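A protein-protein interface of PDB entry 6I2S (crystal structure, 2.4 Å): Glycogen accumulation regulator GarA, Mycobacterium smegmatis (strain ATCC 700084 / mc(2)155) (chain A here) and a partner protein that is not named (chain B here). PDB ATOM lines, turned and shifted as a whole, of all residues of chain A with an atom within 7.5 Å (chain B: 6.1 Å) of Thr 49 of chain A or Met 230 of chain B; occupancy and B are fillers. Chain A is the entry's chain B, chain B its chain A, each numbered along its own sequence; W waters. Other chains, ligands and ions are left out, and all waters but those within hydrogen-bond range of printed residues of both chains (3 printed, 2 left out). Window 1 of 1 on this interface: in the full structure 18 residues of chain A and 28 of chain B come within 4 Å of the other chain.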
ATOM      1  N   ARG A  18       9.654   4.005  11.626  1.00  0.00           N
ATOM      2  CA  ARG A  18       9.621   4.093  10.168  1.00  0.00           C
ATOM      3  C   ARG A  18      10.202   5.456   9.765  1.00  0.00           C
ATOM      4  O   ARG A  18       9.742   6.494  10.241  1.00  0.00           O
ATOM      5  CB  ARG A  18       8.179   3.883   9.670  1.00  0.00           C
ATOM      6  CG  ARG A  18       8.010   3.663   8.185  1.00  0.00           C
ATOM      7  CD  ARG A  18       7.435   2.294   7.848  1.00  0.00           C
ATOM      8  NE  ARG A  18       7.168   2.213   6.410  1.00  0.00           N
ATOM      9  CZ  ARG A  18       6.001   2.502   5.843  1.00  0.00           C
ATOM     10  NH1 ARG A  18       5.872   2.475   4.531  1.00  0.00           N
ATOM     11  NH2 ARG A  18       4.954   2.818   6.589  1.00  0.00           N
ATOM     12  N   ARG A  37      11.725  20.029  10.192  1.00  0.00           N
ATOM     13  CA  ARG A  37      12.900  19.967   9.323  1.00  0.00           C
ATOM     14  C   ARG A  37      13.882  21.149   9.559  1.00  0.00           C
ATOM     15  O   ARG A  37      14.960  21.194   8.955  1.00  0.00           O
ATOM     16  CB  ARG A  37      12.476  19.896   7.857  1.00  0.00           C
ATOM     17  CG  ARG A  37      13.474  19.147   7.021  1.00  0.00           C
ATOM     18  CD  ARG A  37      13.219  19.373   5.564  1.00  0.00           C
ATOM     19  NE  ARG A  37      14.287  18.805   4.754  1.00  0.00           N
ATOM     20  CZ  ARG A  37      14.379  18.943   3.440  1.00  0.00           C
ATOM     21  NH1 ARG A  37      13.471  19.651   2.774  1.00  0.00           N
ATOM     22  NH2 ARG A  37      15.398  18.406   2.781  1.00  0.00           N
ATOM     23  N   LEU A  45      13.712  15.923  12.099  1.00  0.00           N
ATOM     24  CA  LEU A  45      13.269  14.869  11.178  1.00  0.00           C
ATOM     25  C   LEU A  45      13.550  15.320   9.720  1.00  0.00           C
ATOM     26  O   LEU A  45      12.767  16.070   9.135  1.00  0.00           O
ATOM     27  CB  LEU A  45      11.771  14.561  11.417  1.00  0.00           C
ATOM     28  CG  LEU A  45      11.362  14.065  12.814  1.00  0.00           C
ATOM     29  CD1 LEU A  45       9.858  14.040  12.971  1.00  0.00           C
ATOM     30  CD2 LEU A  45      11.949  12.683  13.120  1.00  0.00           C
ATOM     31  N   ASP A  46      14.713  14.910   9.177  1.00  0.00           N
ATOM     32  CA  ASP A  46      15.234  15.339   7.871  1.00  0.00           C
ATOM     33  C   ASP A  46      14.636  14.604   6.645  1.00  0.00           C
ATOM     34  O   ASP A  46      15.117  13.540   6.251  1.00  0.00           O
ATOM     35  CB  ASP A  46      16.763  15.192   7.850  1.00  0.00           C
ATOM     36  CG  ASP A  46      17.485  16.164   6.944  1.00  0.00           C
ATOM     37  OD1 ASP A  46      16.803  16.988   6.287  1.00  0.00           O
ATOM     38  OD2 ASP A  46      18.734  16.127   6.913  1.00  0.00           O
ATOM     39  N   ASP A  47      13.622  15.231   6.014  1.00  0.00           N
ATOM     40  CA  ASP A  47      12.920  14.749   4.824  1.00  0.00           C
ATOM     41  C   ASP A  47      12.035  15.829   4.227  1.00  0.00           C
ATOM     42  O   ASP A  47      11.366  16.564   4.955  1.00  0.00           O
ATOM     43  CB  ASP A  47      12.061  13.510   5.123  1.00  0.00           C
ATOM     44  CG  ASP A  47      11.796  12.683   3.887  1.00  0.00           C
ATOM     45  OD1 ASP A  47      12.740  12.048   3.393  1.00  0.00           O
ATOM     46  OD2 ASP A  47      10.652  12.684   3.410  1.00  0.00           O
ATOM     47  N   VAL A  48      11.977  15.859   2.882  1.00  0.00           N
ATOM     48  CA  VAL A  48      11.203  16.800   2.065  1.00  0.00           C
ATOM     49  C   VAL A  48       9.702  16.751   2.423  1.00  0.00           C
ATOM     50  O   VAL A  48       9.013  17.735   2.196  1.00  0.00           O
ATOM     51  CB  VAL A  48      11.438  16.603   0.538  1.00  0.00           C
ATOM     52  CG1 VAL A  48      12.854  17.013   0.136  1.00  0.00           C
ATOM     53  CG2 VAL A  48      11.129  15.177   0.079  1.00  0.00           C
ATOM     54  N   THR A  49       9.223  15.647   3.034  1.00  0.00           N
ATOM     55  CA  THR A  49       7.826  15.451   3.453  1.00  0.00           C
ATOM     56  C   THR A  49       7.509  16.134   4.796  1.00  0.00           C
ATOM     57  O   THR A  49       6.346  16.363   5.114  1.00  0.00           O
ATOM     58  CB  THR A  49       7.497  13.963   3.533  1.00  0.00           C
ATOM     59  OG1 THR A  49       8.303  13.345   4.536  1.00  0.00           O
ATOM     60  CG2 THR A  49       7.628  13.251   2.178  1.00  0.00           C
ATOM     61  N   VAL A  50       8.544  16.445   5.578  1.00  0.00           N
ATOM     62  CA  VAL A  50       8.436  17.122   6.860  1.00  0.00           C
ATOM     63  C   VAL A  50       8.655  18.633   6.607  1.00  0.00           C
ATOM     64  O   VAL A  50       9.608  19.003   5.916  1.00  0.00           O
ATOM     65  CB  VAL A  50       9.456  16.524   7.860  1.00  0.00           C
ATOM     66  CG1 VAL A  50       9.437  17.270   9.195  1.00  0.00           C
ATOM     67  CG2 VAL A  50       9.206  15.039   8.064  1.00  0.00           C
ATOM     68  N   SER A  51       7.767  19.491   7.143  1.00  0.00           N
ATOM     69  CA  SER A  51       7.863  20.945   6.980  1.00  0.00           C
ATOM     70  C   SER A  51       8.897  21.548   7.961  1.00  0.00           C
ATOM     71  O   SER A  51       9.171  20.938   9.002  1.00  0.00           O
ATOM     72  CB  SER A  51       6.495  21.589   7.183  1.00  0.00           C
ATOM     73  OG  SER A  51       5.604  21.244   6.137  1.00  0.00           O
ATOM     74  N   ARG A  52       9.457  22.740   7.611  1.00  0.00           N
ATOM     75  CA  ARG A  52      10.426  23.494   8.419  1.00  0.00           C
ATOM     76  C   ARG A  52       9.973  23.506   9.888  1.00  0.00           C
ATOM     77  O   ARG A  52      10.744  23.163  10.794  1.00  0.00           O
ATOM     78  CB  ARG A  52      10.573  24.932   7.863  1.00  0.00           C
ATOM     79  CG  ARG A  52      11.617  25.822   8.558  1.00  0.00           C
ATOM     80  CD  ARG A  52      13.010  25.649   7.976  1.00  0.00           C
ATOM     81  NE  ARG A  52      13.798  26.881   8.039  1.00  0.00           N
ATOM     82  CZ  ARG A  52      15.127  26.925   7.990  1.00  0.00           C
ATOM     83  NH1 ARG A  52      15.833  25.805   7.895  1.00  0.00           N
ATOM     84  NH2 ARG A  52      15.759  28.086   8.053  1.00  0.00           N
ATOM     85  N   HIS A  54       6.820  21.812  11.814  1.00  0.00           N
ATOM     86  CA  HIS A  54       5.801  20.811  11.548  1.00  0.00           C
ATOM     87  C   HIS A  54       4.882  20.526  12.731  1.00  0.00           C
ATOM     88  O   HIS A  54       3.667  20.697  12.628  1.00  0.00           O
ATOM     89  CB  HIS A  54       6.487  19.507  11.106  1.00  0.00           C
ATOM     90  CG  HIS A  54       5.600  18.586  10.337  1.00  0.00           C
ATOM     91  ND1 HIS A  54       5.794  18.367   9.001  1.00  0.00           N
ATOM     92  CD2 HIS A  54       4.542  17.854  10.754  1.00  0.00           C
ATOM     93  CE1 HIS A  54       4.860  17.504   8.643  1.00  0.00           C
ATOM     94  NE2 HIS A  54       4.078  17.179   9.670  1.00  0.00           N
ATOM     95  N   SER A  71       1.981  22.624   9.259  1.00  0.00           N
ATOM     96  CA  SER A  71       2.706  21.816   8.289  1.00  0.00           C
ATOM     97  C   SER A  71       1.851  21.614   7.050  1.00  0.00           C
ATOM     98  O   SER A  71       0.623  21.745   7.114  1.00  0.00           O
ATOM     99  CB  SER A  71       3.082  20.476   8.901  1.00  0.00           C
ATOM    100  OG  SER A  71       2.025  19.533   8.823  1.00  0.00           O
ATOM    101  N   LEU A  72       2.496  21.296   5.928  1.00  0.00           N
ATOM    102  CA  LEU A  72       1.800  21.037   4.689  1.00  0.00           C
ATOM    103  C   LEU A  72       1.201  19.625   4.690  1.00  0.00           C
ATOM    104  O   LEU A  72       0.060  19.469   4.253  1.00  0.00           O
ATOM    105  CB  LEU A  72       2.761  21.229   3.494  1.00  0.00           C
ATOM    106  CG  LEU A  72       2.265  20.910   2.064  1.00  0.00           C
ATOM    107  CD1 LEU A  72       0.959  21.641   1.724  1.00  0.00           C
ATOM    108  CD2 LEU A  72       3.307  21.301   1.052  1.00  0.00           C
ATOM    109  N   ASN A  73       1.963  18.607   5.155  1.00  0.00           N
ATOM    110  CA  ASN A  73       1.524  17.204   5.094  1.00  0.00           C
ATOM    111  C   ASN A  73       0.730  16.723   6.336  1.00  0.00           C
ATOM    112  O   ASN A  73       0.233  15.597   6.337  1.00  0.00           O
ATOM    113  CB  ASN A  73       2.715  16.262   4.826  1.00  0.00           C
ATOM    114  CG  ASN A  73       3.129  16.225   3.369  1.00  0.00           C
ATOM    115  OD1 ASN A  73       2.300  16.310   2.462  1.00  0.00           O
ATOM    116  ND2 ASN A  73       4.420  16.083   3.111  1.00  0.00           N
ATOM    117  N   GLY A  74       0.585  17.592   7.335  1.00  0.00           N
ATOM    118  CA  GLY A  74      -0.164  17.307   8.554  1.00  0.00           C
ATOM    119  C   GLY A  74       0.505  16.394   9.563  1.00  0.00           C
ATOM    120  O   GLY A  74       1.642  15.956   9.384  1.00  0.00           O
ATOM    121  N   TYR A  76      -0.459  12.940  12.079  1.00  0.00           N
ATOM    122  CA  TYR A  76      -1.385  11.824  12.251  1.00  0.00           C
ATOM    123  C   TYR A  76      -1.118  11.132  13.571  1.00  0.00           C
ATOM    124  O   TYR A  76       0.040  11.025  13.979  1.00  0.00           O
ATOM    125  CB  TYR A  76      -1.260  10.798  11.096  1.00  0.00           C
ATOM    126  CG  TYR A  76      -1.646  11.327   9.729  1.00  0.00           C
ATOM    127  CD1 TYR A  76      -0.777  12.139   9.002  1.00  0.00           C
ATOM    128  CD2 TYR A  76      -2.857  10.976   9.140  1.00  0.00           C
ATOM    129  CE1 TYR A  76      -1.136  12.652   7.757  1.00  0.00           C
ATOM    130  CE2 TYR A  76      -3.204  11.438   7.868  1.00  0.00           C
ATOM    131  CZ  TYR A  76      -2.343  12.284   7.182  1.00  0.00           C
ATOM    132  OH  TYR A  76      -2.690  12.779   5.944  1.00  0.00           O
ATOM    133  N   ARG A  79      -2.928   6.688  12.458  1.00  0.00           N
ATOM    134  CA  ARG A  79      -3.441   6.806  11.071  1.00  0.00           C
ATOM    135  C   ARG A  79      -4.621   7.813  10.921  1.00  0.00           C
ATOM    136  O   ARG A  79      -5.269   7.839   9.875  1.00  0.00           O
ATOM    137  CB  ARG A  79      -3.847   5.420  10.480  1.00  0.00           C
ATOM    138  CG  ARG A  79      -2.764   4.332  10.507  1.00  0.00           C
ATOM    139  CD  ARG A  79      -1.466   4.740   9.803  1.00  0.00           C
ATOM    140  NE  ARG A  79      -1.531   4.608   8.341  1.00  0.00           N
ATOM    141  CZ  ARG A  79      -1.212   3.505   7.672  1.00  0.00           C
ATOM    142  NH1 ARG A  79      -1.282   3.482   6.350  1.00  0.00           N
ATOM    143  NH2 ARG A  79      -0.832   2.411   8.322  1.00  0.00           N
ATOM    144  N   GLN A  94       2.627  10.249  13.028  1.00  0.00           N
ATOM    145  CA  GLN A  94       3.230  10.351  11.708  1.00  0.00           C
ATOM    146  C   GLN A  94       3.525  11.816  11.393  1.00  0.00           C
ATOM    147  O   GLN A  94       2.610  12.642  11.379  1.00  0.00           O
ATOM    148  CB  GLN A  94       2.350   9.715  10.623  1.00  0.00           C
ATOM    149  CG  GLN A  94       3.047   9.643   9.264  1.00  0.00           C
ATOM    150  CD  GLN A  94       2.244   8.962   8.193  1.00  0.00           C
ATOM    151  OE1 GLN A  94       1.235   8.291   8.450  1.00  0.00           O
ATOM    152  NE2 GLN A  94       2.681   9.125   6.956  1.00  0.00           N
ATOM    153  N   ILE A  95       4.808  12.127  11.155  1.00  0.00           N
ATOM    154  CA  ILE A  95       5.282  13.467  10.795  1.00  0.00           C
ATOM    155  C   ILE A  95       6.028  13.278   9.489  1.00  0.00           C
ATOM    156  O   ILE A  95       7.126  12.720   9.495  1.00  0.00           O
ATOM    157  CB  ILE A  95       6.111  14.153  11.944  1.00  0.00           C
ATOM    158  CG1 ILE A  95       5.190  14.503  13.145  1.00  0.00           C
ATOM    159  CG2 ILE A  95       6.859  15.416  11.444  1.00  0.00           C
ATOM    160  CD1 ILE A  95       5.929  14.702  14.500  1.00  0.00           C
ATOM    161  N   GLY A  96       5.383  13.662   8.380  1.00  0.00           N
ATOM    162  CA  GLY A  96       5.900  13.424   7.039  1.00  0.00           C
ATOM    163  C   GLY A  96       5.934  11.920   6.820  1.00  0.00           C
ATOM    164  O   GLY A  96       4.981  11.237   7.198  1.00  0.00           O
ATOM    165  N   LYS A  97       7.044  11.371   6.289  1.00  0.00           N
ATOM    166  CA  LYS A  97       7.184   9.916   6.101  1.00  0.00           C
ATOM    167  C   LYS A  97       7.580   9.161   7.408  1.00  0.00           C
ATOM    168  O   LYS A  97       7.625   7.929   7.420  1.00  0.00           O
ATOM    169  CB  LYS A  97       8.219   9.627   5.016  1.00  0.00           C
ATOM    170  CG  LYS A  97       7.548   9.207   3.746  1.00  0.00           C
ATOM    171  CD  LYS A  97       8.236   9.779   2.557  1.00  0.00           C
ATOM    172  CE  LYS A  97       7.408   9.614   1.302  1.00  0.00           C
ATOM    173  NZ  LYS A  97       8.292   9.303   0.174  1.00  0.00           N
ATOM    174  N   PHE A  98       7.896   9.903   8.481  1.00  0.00           N
ATOM    175  CA  PHE A  98       8.319   9.335   9.761  1.00  0.00           C
ATOM    176  C   PHE A  98       7.155   8.872  10.589  1.00  0.00           C
ATOM    177  O   PHE A  98       6.141   9.551  10.680  1.00  0.00           O
ATOM    178  CB  PHE A  98       9.130  10.354  10.587  1.00  0.00           C
ATOM    179  CG  PHE A  98      10.425  10.801   9.960  1.00  0.00           C
ATOM    180  CD1 PHE A  98      10.455  11.875   9.080  1.00  0.00           C
ATOM    181  CD2 PHE A  98      11.624  10.179  10.286  1.00  0.00           C
ATOM    182  CE1 PHE A  98      11.659  12.307   8.520  1.00  0.00           C
ATOM    183  CE2 PHE A  98      12.830  10.623   9.732  1.00  0.00           C
ATOM    184  CZ  PHE A  98      12.839  11.682   8.853  1.00  0.00           C
ATOM    185  N   ARG A  99       7.325   7.721  11.217  1.00  0.00           N
ATOM    186  CA  ARG A  99       6.359   7.113  12.129  1.00  0.00           C
ATOM    187  C   ARG A  99       7.090   6.912  13.449  1.00  0.00           C
ATOM    188  O   ARG A  99       8.105   6.222  13.504  1.00  0.00           O
ATOM    189  CB  ARG A  99       5.763   5.811  11.531  1.00  0.00           C
ATOM    190  CG  ARG A  99       4.559   6.101  10.626  1.00  0.00           C
ATOM    191  CD  ARG A  99       4.476   5.285   9.361  1.00  0.00           C
ATOM    192  NE  ARG A  99       5.226   5.916   8.279  1.00  0.00           N
ATOM    193  CZ  ARG A  99       4.819   6.026   7.017  1.00  0.00           C
ATOM    194  NH1 ARG A  99       3.644   5.527   6.641  1.00  0.00           N
ATOM    195  NH2 ARG A  99       5.584   6.626   6.120  1.00  0.00           N
ATOM    196  N   TYR B 122       0.150  16.361  -0.643  1.00  0.00           N
ATOM    197  CA  TYR B 122       1.329  15.523  -0.828  1.00  0.00           C
ATOM    198  C   TYR B 122       1.965  15.811  -2.227  1.00  0.00           C
ATOM    199  O   TYR B 122       3.184  15.998  -2.306  1.00  0.00           O
ATOM    200  CB  TYR B 122       1.015  14.023  -0.609  1.00  0.00           C
ATOM    201  CG  TYR B 122       2.254  13.162  -0.773  1.00  0.00           C
ATOM    202  CD1 TYR B 122       3.289  13.205   0.166  1.00  0.00           C
ATOM    203  CD2 TYR B 122       2.459  12.412  -1.935  1.00  0.00           C
ATOM    204  CE1 TYR B 122       4.466  12.481  -0.020  1.00  0.00           C
ATOM    205  CE2 TYR B 122       3.638  11.704  -2.137  1.00  0.00           C
ATOM    206  CZ  TYR B 122       4.629  11.723  -1.169  1.00  0.00           C
ATOM    207  OH  TYR B 122       5.794  11.031  -1.371  1.00  0.00           O
ATOM    208  N   SER B 125       3.685  19.096  -2.018  1.00  0.00           N
ATOM    209  CA  SER B 125       4.938  19.000  -1.253  1.00  0.00           C
ATOM    210  C   SER B 125       6.096  18.498  -2.149  1.00  0.00           C
ATOM    211  O   SER B 125       7.227  18.948  -1.971  1.00  0.00           O
ATOM    212  CB  SER B 125       4.765  18.125  -0.009  1.00  0.00           C
ATOM    213  OG  SER B 125       4.829  16.740  -0.296  1.00  0.00           O
ATOM    214  N   LYS B 126       5.788  17.612  -3.132  1.00  0.00           N
ATOM    215  CA  LYS B 126       6.728  17.075  -4.113  1.00  0.00           C
ATOM    216  C   LYS B 126       7.061  18.131  -5.185  1.00  0.00           C
ATOM    217  O   LYS B 126       8.223  18.210  -5.588  1.00  0.00           O
ATOM    218  CB  LYS B 126       6.232  15.750  -4.726  1.00  0.00           C
ATOM    219  CG  LYS B 126       6.542  14.509  -3.849  1.00  0.00           C
ATOM    220  CD  LYS B 126       8.066  14.246  -3.692  1.00  0.00           C
ATOM    221  CE  LYS B 126       8.465  13.204  -2.676  1.00  0.00           C
ATOM    222  NZ  LYS B 126       8.091  13.579  -1.295  1.00  0.00           N
ATOM    223  N   ASP B 164       5.467   4.552  -5.620  1.00  0.00           N
ATOM    224  CA  ASP B 164       4.468   4.348  -4.580  1.00  0.00           C
ATOM    225  C   ASP B 164       3.509   3.228  -4.971  1.00  0.00           C
ATOM    226  O   ASP B 164       3.254   2.336  -4.152  1.00  0.00           O
ATOM    227  CB  ASP B 164       3.699   5.645  -4.304  1.00  0.00           C
ATOM    228  CG  ASP B 164       2.651   5.435  -3.244  1.00  0.00           C
ATOM    229  OD1 ASP B 164       3.027   5.216  -2.076  1.00  0.00           O
ATOM    230  OD2 ASP B 164       1.463   5.432  -3.590  1.00  0.00           O
ATOM    231  N   TYR B 227      12.662   3.850  -0.726  1.00  0.00           N
ATOM    232  CA  TYR B 227      11.458   4.642  -0.800  1.00  0.00           C
ATOM    233  C   TYR B 227      10.470   4.124   0.264  1.00  0.00           C
ATOM    234  O   TYR B 227      10.213   2.918   0.333  1.00  0.00           O
ATOM    235  CB  TYR B 227      10.859   4.585  -2.206  1.00  0.00           C
ATOM    236  CG  TYR B 227       9.606   5.415  -2.344  1.00  0.00           C
ATOM    237  CD1 TYR B 227       8.368   4.930  -1.913  1.00  0.00           C
ATOM    238  CD2 TYR B 227       9.652   6.692  -2.889  1.00  0.00           C
ATOM    239  CE1 TYR B 227       7.215   5.701  -2.016  1.00  0.00           C
ATOM    240  CE2 TYR B 227       8.503   7.474  -2.990  1.00  0.00           C
ATOM    241  CZ  TYR B 227       7.287   6.971  -2.558  1.00  0.00           C
ATOM    242  OH  TYR B 227       6.169   7.753  -2.624  1.00  0.00           O
ATOM    243  N   ILE B 228       9.920   5.045   1.071  1.00  0.00           N
ATOM    244  CA  ILE B 228       8.932   4.784   2.122  1.00  0.00           C
ATOM    245  C   ILE B 228       7.590   5.400   1.685  1.00  0.00           C
ATOM    246  O   ILE B 228       7.548   6.567   1.320  1.00  0.00           O
ATOM    247  CB  ILE B 228       9.433   5.329   3.505  1.00  0.00           C
ATOM    248  CG1 ILE B 228      10.700   4.554   3.966  1.00  0.00           C
ATOM    249  CG2 ILE B 228       8.333   5.273   4.587  1.00  0.00           C
ATOM    250  CD1 ILE B 228      11.463   5.176   5.114  1.00  0.00           C
ATOM    251  N   GLN B 229       6.506   4.616   1.682  1.00  0.00           N
ATOM    252  CA  GLN B 229       5.196   5.141   1.299  1.00  0.00           C
ATOM    253  C   GLN B 229       4.691   6.152   2.336  1.00  0.00           C
ATOM    254  O   GLN B 229       4.879   5.947   3.534  1.00  0.00           O
ATOM    255  CB  GLN B 229       4.180   4.009   1.169  1.00  0.00           C
ATOM    256  CG  GLN B 229       4.388   3.034   0.019  1.00  0.00           C
ATOM    257  CD  GLN B 229       3.188   2.144  -0.067  1.00  0.00           C
ATOM    258  OE1 GLN B 229       3.000   1.210   0.730  1.00  0.00           O
ATOM    259  NE2 GLN B 229       2.329   2.439  -1.020  1.00  0.00           N
ATOM    260  N   MET B 230       4.038   7.217   1.874  1.00  0.00           N
ATOM    261  CA  MET B 230       3.463   8.274   2.705  1.00  0.00           C
ATOM    262  C   MET B 230       2.120   7.851   3.348  1.00  0.00           C
ATOM    263  O   MET B 230       1.809   8.265   4.451  1.00  0.00           O
ATOM    264  CB  MET B 230       3.270   9.540   1.843  1.00  0.00           C
ATOM    265  CG  MET B 230       2.580  10.701   2.536  1.00  0.00           C
ATOM    266  SD  MET B 230       3.341  11.388   4.036  1.00  0.00           S
ATOM    267  CE  MET B 230       4.864  11.627   3.524  1.00  0.00           C
ATOM    268  N   PHE B 231       1.325   7.078   2.659  1.00  0.00           N
ATOM    269  CA  PHE B 231       0.020   6.672   3.160  1.00  0.00           C
ATOM    270  C   PHE B 231      -0.077   5.144   3.291  1.00  0.00           C
ATOM    271  O   PHE B 231      -1.066   4.640   3.813  1.00  0.00           O
ATOM    272  CB  PHE B 231      -1.080   7.226   2.234  1.00  0.00           C
ATOM    273  CG  PHE B 231      -0.998   8.727   2.076  1.00  0.00           C
ATOM    274  CD1 PHE B 231      -1.263   9.575   3.153  1.00  0.00           C
ATOM    275  CD2 PHE B 231      -0.592   9.296   0.870  1.00  0.00           C
ATOM    276  CE1 PHE B 231      -1.150  10.966   3.015  1.00  0.00           C
ATOM    277  CE2 PHE B 231      -0.511  10.688   0.725  1.00  0.00           C
ATOM    278  CZ  PHE B 231      -0.780  11.511   1.801  1.00  0.00           C
ATOM    279  N   GLY B 232       0.965   4.438   2.865  1.00  0.00           N
ATOM    280  CA  GLY B 232       1.002   2.982   2.889  1.00  0.00           C
ATOM    281  C   GLY B 232       1.939   2.423   3.928  1.00  0.00           C
ATOM    282  O   GLY B 232       2.648   3.165   4.621  1.00  0.00           O
ATOM    283  N   ASP B 436       6.249  25.972   3.583  1.00  0.00           N
ATOM    284  CA  ASP B 436       6.914  24.697   3.352  1.00  0.00           C
ATOM    285  C   ASP B 436       7.933  24.849   2.256  1.00  0.00           C
ATOM    286  O   ASP B 436       9.056  24.386   2.437  1.00  0.00           O
ATOM    287  CB  ASP B 436       5.894  23.600   3.003  1.00  0.00           C
ATOM    288  CG  ASP B 436       6.532  22.263   2.703  1.00  0.00           C
ATOM    289  OD1 ASP B 436       6.898  22.031   1.532  1.00  0.00           O
ATOM    290  OD2 ASP B 436       6.678  21.452   3.641  1.00  0.00           O
ATOM    291  N   GLN B 440      11.922  24.295   2.215  1.00  0.00           N
ATOM    292  CA  GLN B 440      12.593  23.337   1.316  1.00  0.00           C
ATOM    293  C   GLN B 440      13.825  23.974   0.694  1.00  0.00           C
ATOM    294  O   GLN B 440      14.831  23.305   0.453  1.00  0.00           O
ATOM    295  CB  GLN B 440      11.666  22.860   0.172  1.00  0.00           C
ATOM    296  CG  GLN B 440      10.335  22.266   0.588  1.00  0.00           C
ATOM    297  CD  GLN B 440      10.318  20.767   0.585  1.00  0.00           C
ATOM    298  OE1 GLN B 440      11.310  20.096   0.285  1.00  0.00           O
ATOM    299  NE2 GLN B 440       9.173  20.215   0.923  1.00  0.00           N
HETATM  300  O   HOH W   1       7.351  15.921   0.142  1.00  0.00           O
HETATM  301  O   HOH W   2       9.650  23.078   4.736  1.00  0.00           O
HETATM  302  O   HOH W   3      10.671  20.494   4.023  1.00  0.00           O
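Water W3 lies within hydrogen-bond range of the backbone carbonyl oxygen (O) of Val 50 of chain A (2.6 Å), the guanidinium group (NH1) of Arg 37 of chain A (3.2 Å) and the side-chain amide nitrogen (NE2) of Gln 440 of chain B (3.5 Å).
Water W2 lies within hydrogen-bond range of O of Asp 436 of chain B (2.7 Å) and N of Arg 52 of chain A (2.9 Å).
Printed residues of chain B within 4 Å of Arg 37 of chain A: Gln 440 (3.3 Å).
Leu 45 of chain A touches none of the printed residues of chain B.
Printed residues of chain A within 4 Å of Tyr 227 of chain B: Lys 97.
Printed residues of chain A within 4 Å of Gly 232 of chain B: Arg 18 and Arg 99.
The nearest residue of chain B that does not touch Thr 49 of chain A is Ser 125 of chain B (5.0 Å).
The nearest residue of chain A that does not touch Met 230 of chain B is Asn 73 of chain A (4.5 Å).
NH1 of Arg 18 of chain A touches N of Gln 229 of chain B, 3.6 Å away.
CG2 of Thr 49 of chain A touches CE1 of Tyr 122 of chain B, at 3.9 Å.
Lys 126 of chain B touches Thr 49 of chain A (NZ to CG2, 3.5 Å).
Thr 49 of chain A touches Met 230 of chain B.
NH1 of Arg 99 of chain A touches O of Met 230 of chain B, 3.96 Å away.
The side-chain hydroxyl of Tyr 122 of chain B lies within hydrogen-bond range of the side-chain amino group of Lys 97 of chain A, 3.4 Å away.
The side-chain hydroxyl (OG) of Ser 125 of chain B lies within hydrogen-bond range of the side-chain amide nitrogen (ND2) of Asn 73 of chain A, 3.5 Å away.
O of Ile 228 of chain B lies close to NZ of Lys 97 of chain A, at 3.1 Å.
The backbone carbonyl oxygen (O) of Gln 229 of chain B is in hydrogen-bond range of the guanidinium group (NH2) of Arg 99 of chain A, at 2.8 Å.
The backbone carbonyl oxygen (O) of Met 230 of chain B lies within hydrogen-bond range of the side-chain amide nitrogen (NE2) of Gln 94 of chain A, at 2.8 Å.
The backbone carbonyl oxygen of Phe 231 of chain B lies within hydrogen-bond range of the guanidinium group of Arg 79 of chain A (2.8 Å).
The backbone carbonyl oxygen of Gly 232 of chain B is in hydrogen-bond range of the guanidinium group of Arg 18 of chain A (3.1 Å).
The guanidinium group (NH1) of Arg 99 of chain A is in hydrogen-bond range of the backbone carbonyl oxygen (O) of Gly 232 of chain B (3.3 Å).
The side-chain carboxylate (OD2) of Asp 436 of chain B lies within hydrogen-bond range of the side-chain hydroxyl (OG) of Ser 51 of chain A.
OE1 of Gln 440 of chain B sits at hydrogen-bond distance from NH1 of Arg 37 of chain A (3.3 Å).
NE2 of Gln 440 of chain B sits at hydrogen-bond distance from O of Val 48 of chain A (2.8 Å).
The backbone carbonyl oxygen (O) of Gly 96 of chain A sits close to the side-chain sulfur (SD) of Met 230 of chain B (3.6 Å).
Printed residues of chain A that touch a printed residue of chain B: Arg 18, Arg 37, Val 48, Thr 49, Ser 51, Leu 72, Asn 73, Tyr 76, Arg 79, Gln 94, Gly 96, Lys 97 and Arg 99.
Of the 12 printed residues of chain B, 11 touch a printed residue of chain A.
Among the printed residues, no Asp or Glu carboxylate lies within 4 Å of a Lys or Arg side-chain nitrogen of the other chain.
The side-chain amino group (NZ) of Lys 126 of chain B is in hydrogen-bond range of the side-chain hydroxyl (OH) of Tyr 122 of chain B, 3.4 Å away.
NE of Arg 37 of chain A is in salt-bridge range of OD1 of Asp 46 of chain A (3.5 Å).
The backbone NH (N) of Ser 51 of chain A lies within hydrogen-bond range of a ring nitrogen (ND1) of His 54 of chain A, at 2.9 Å.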
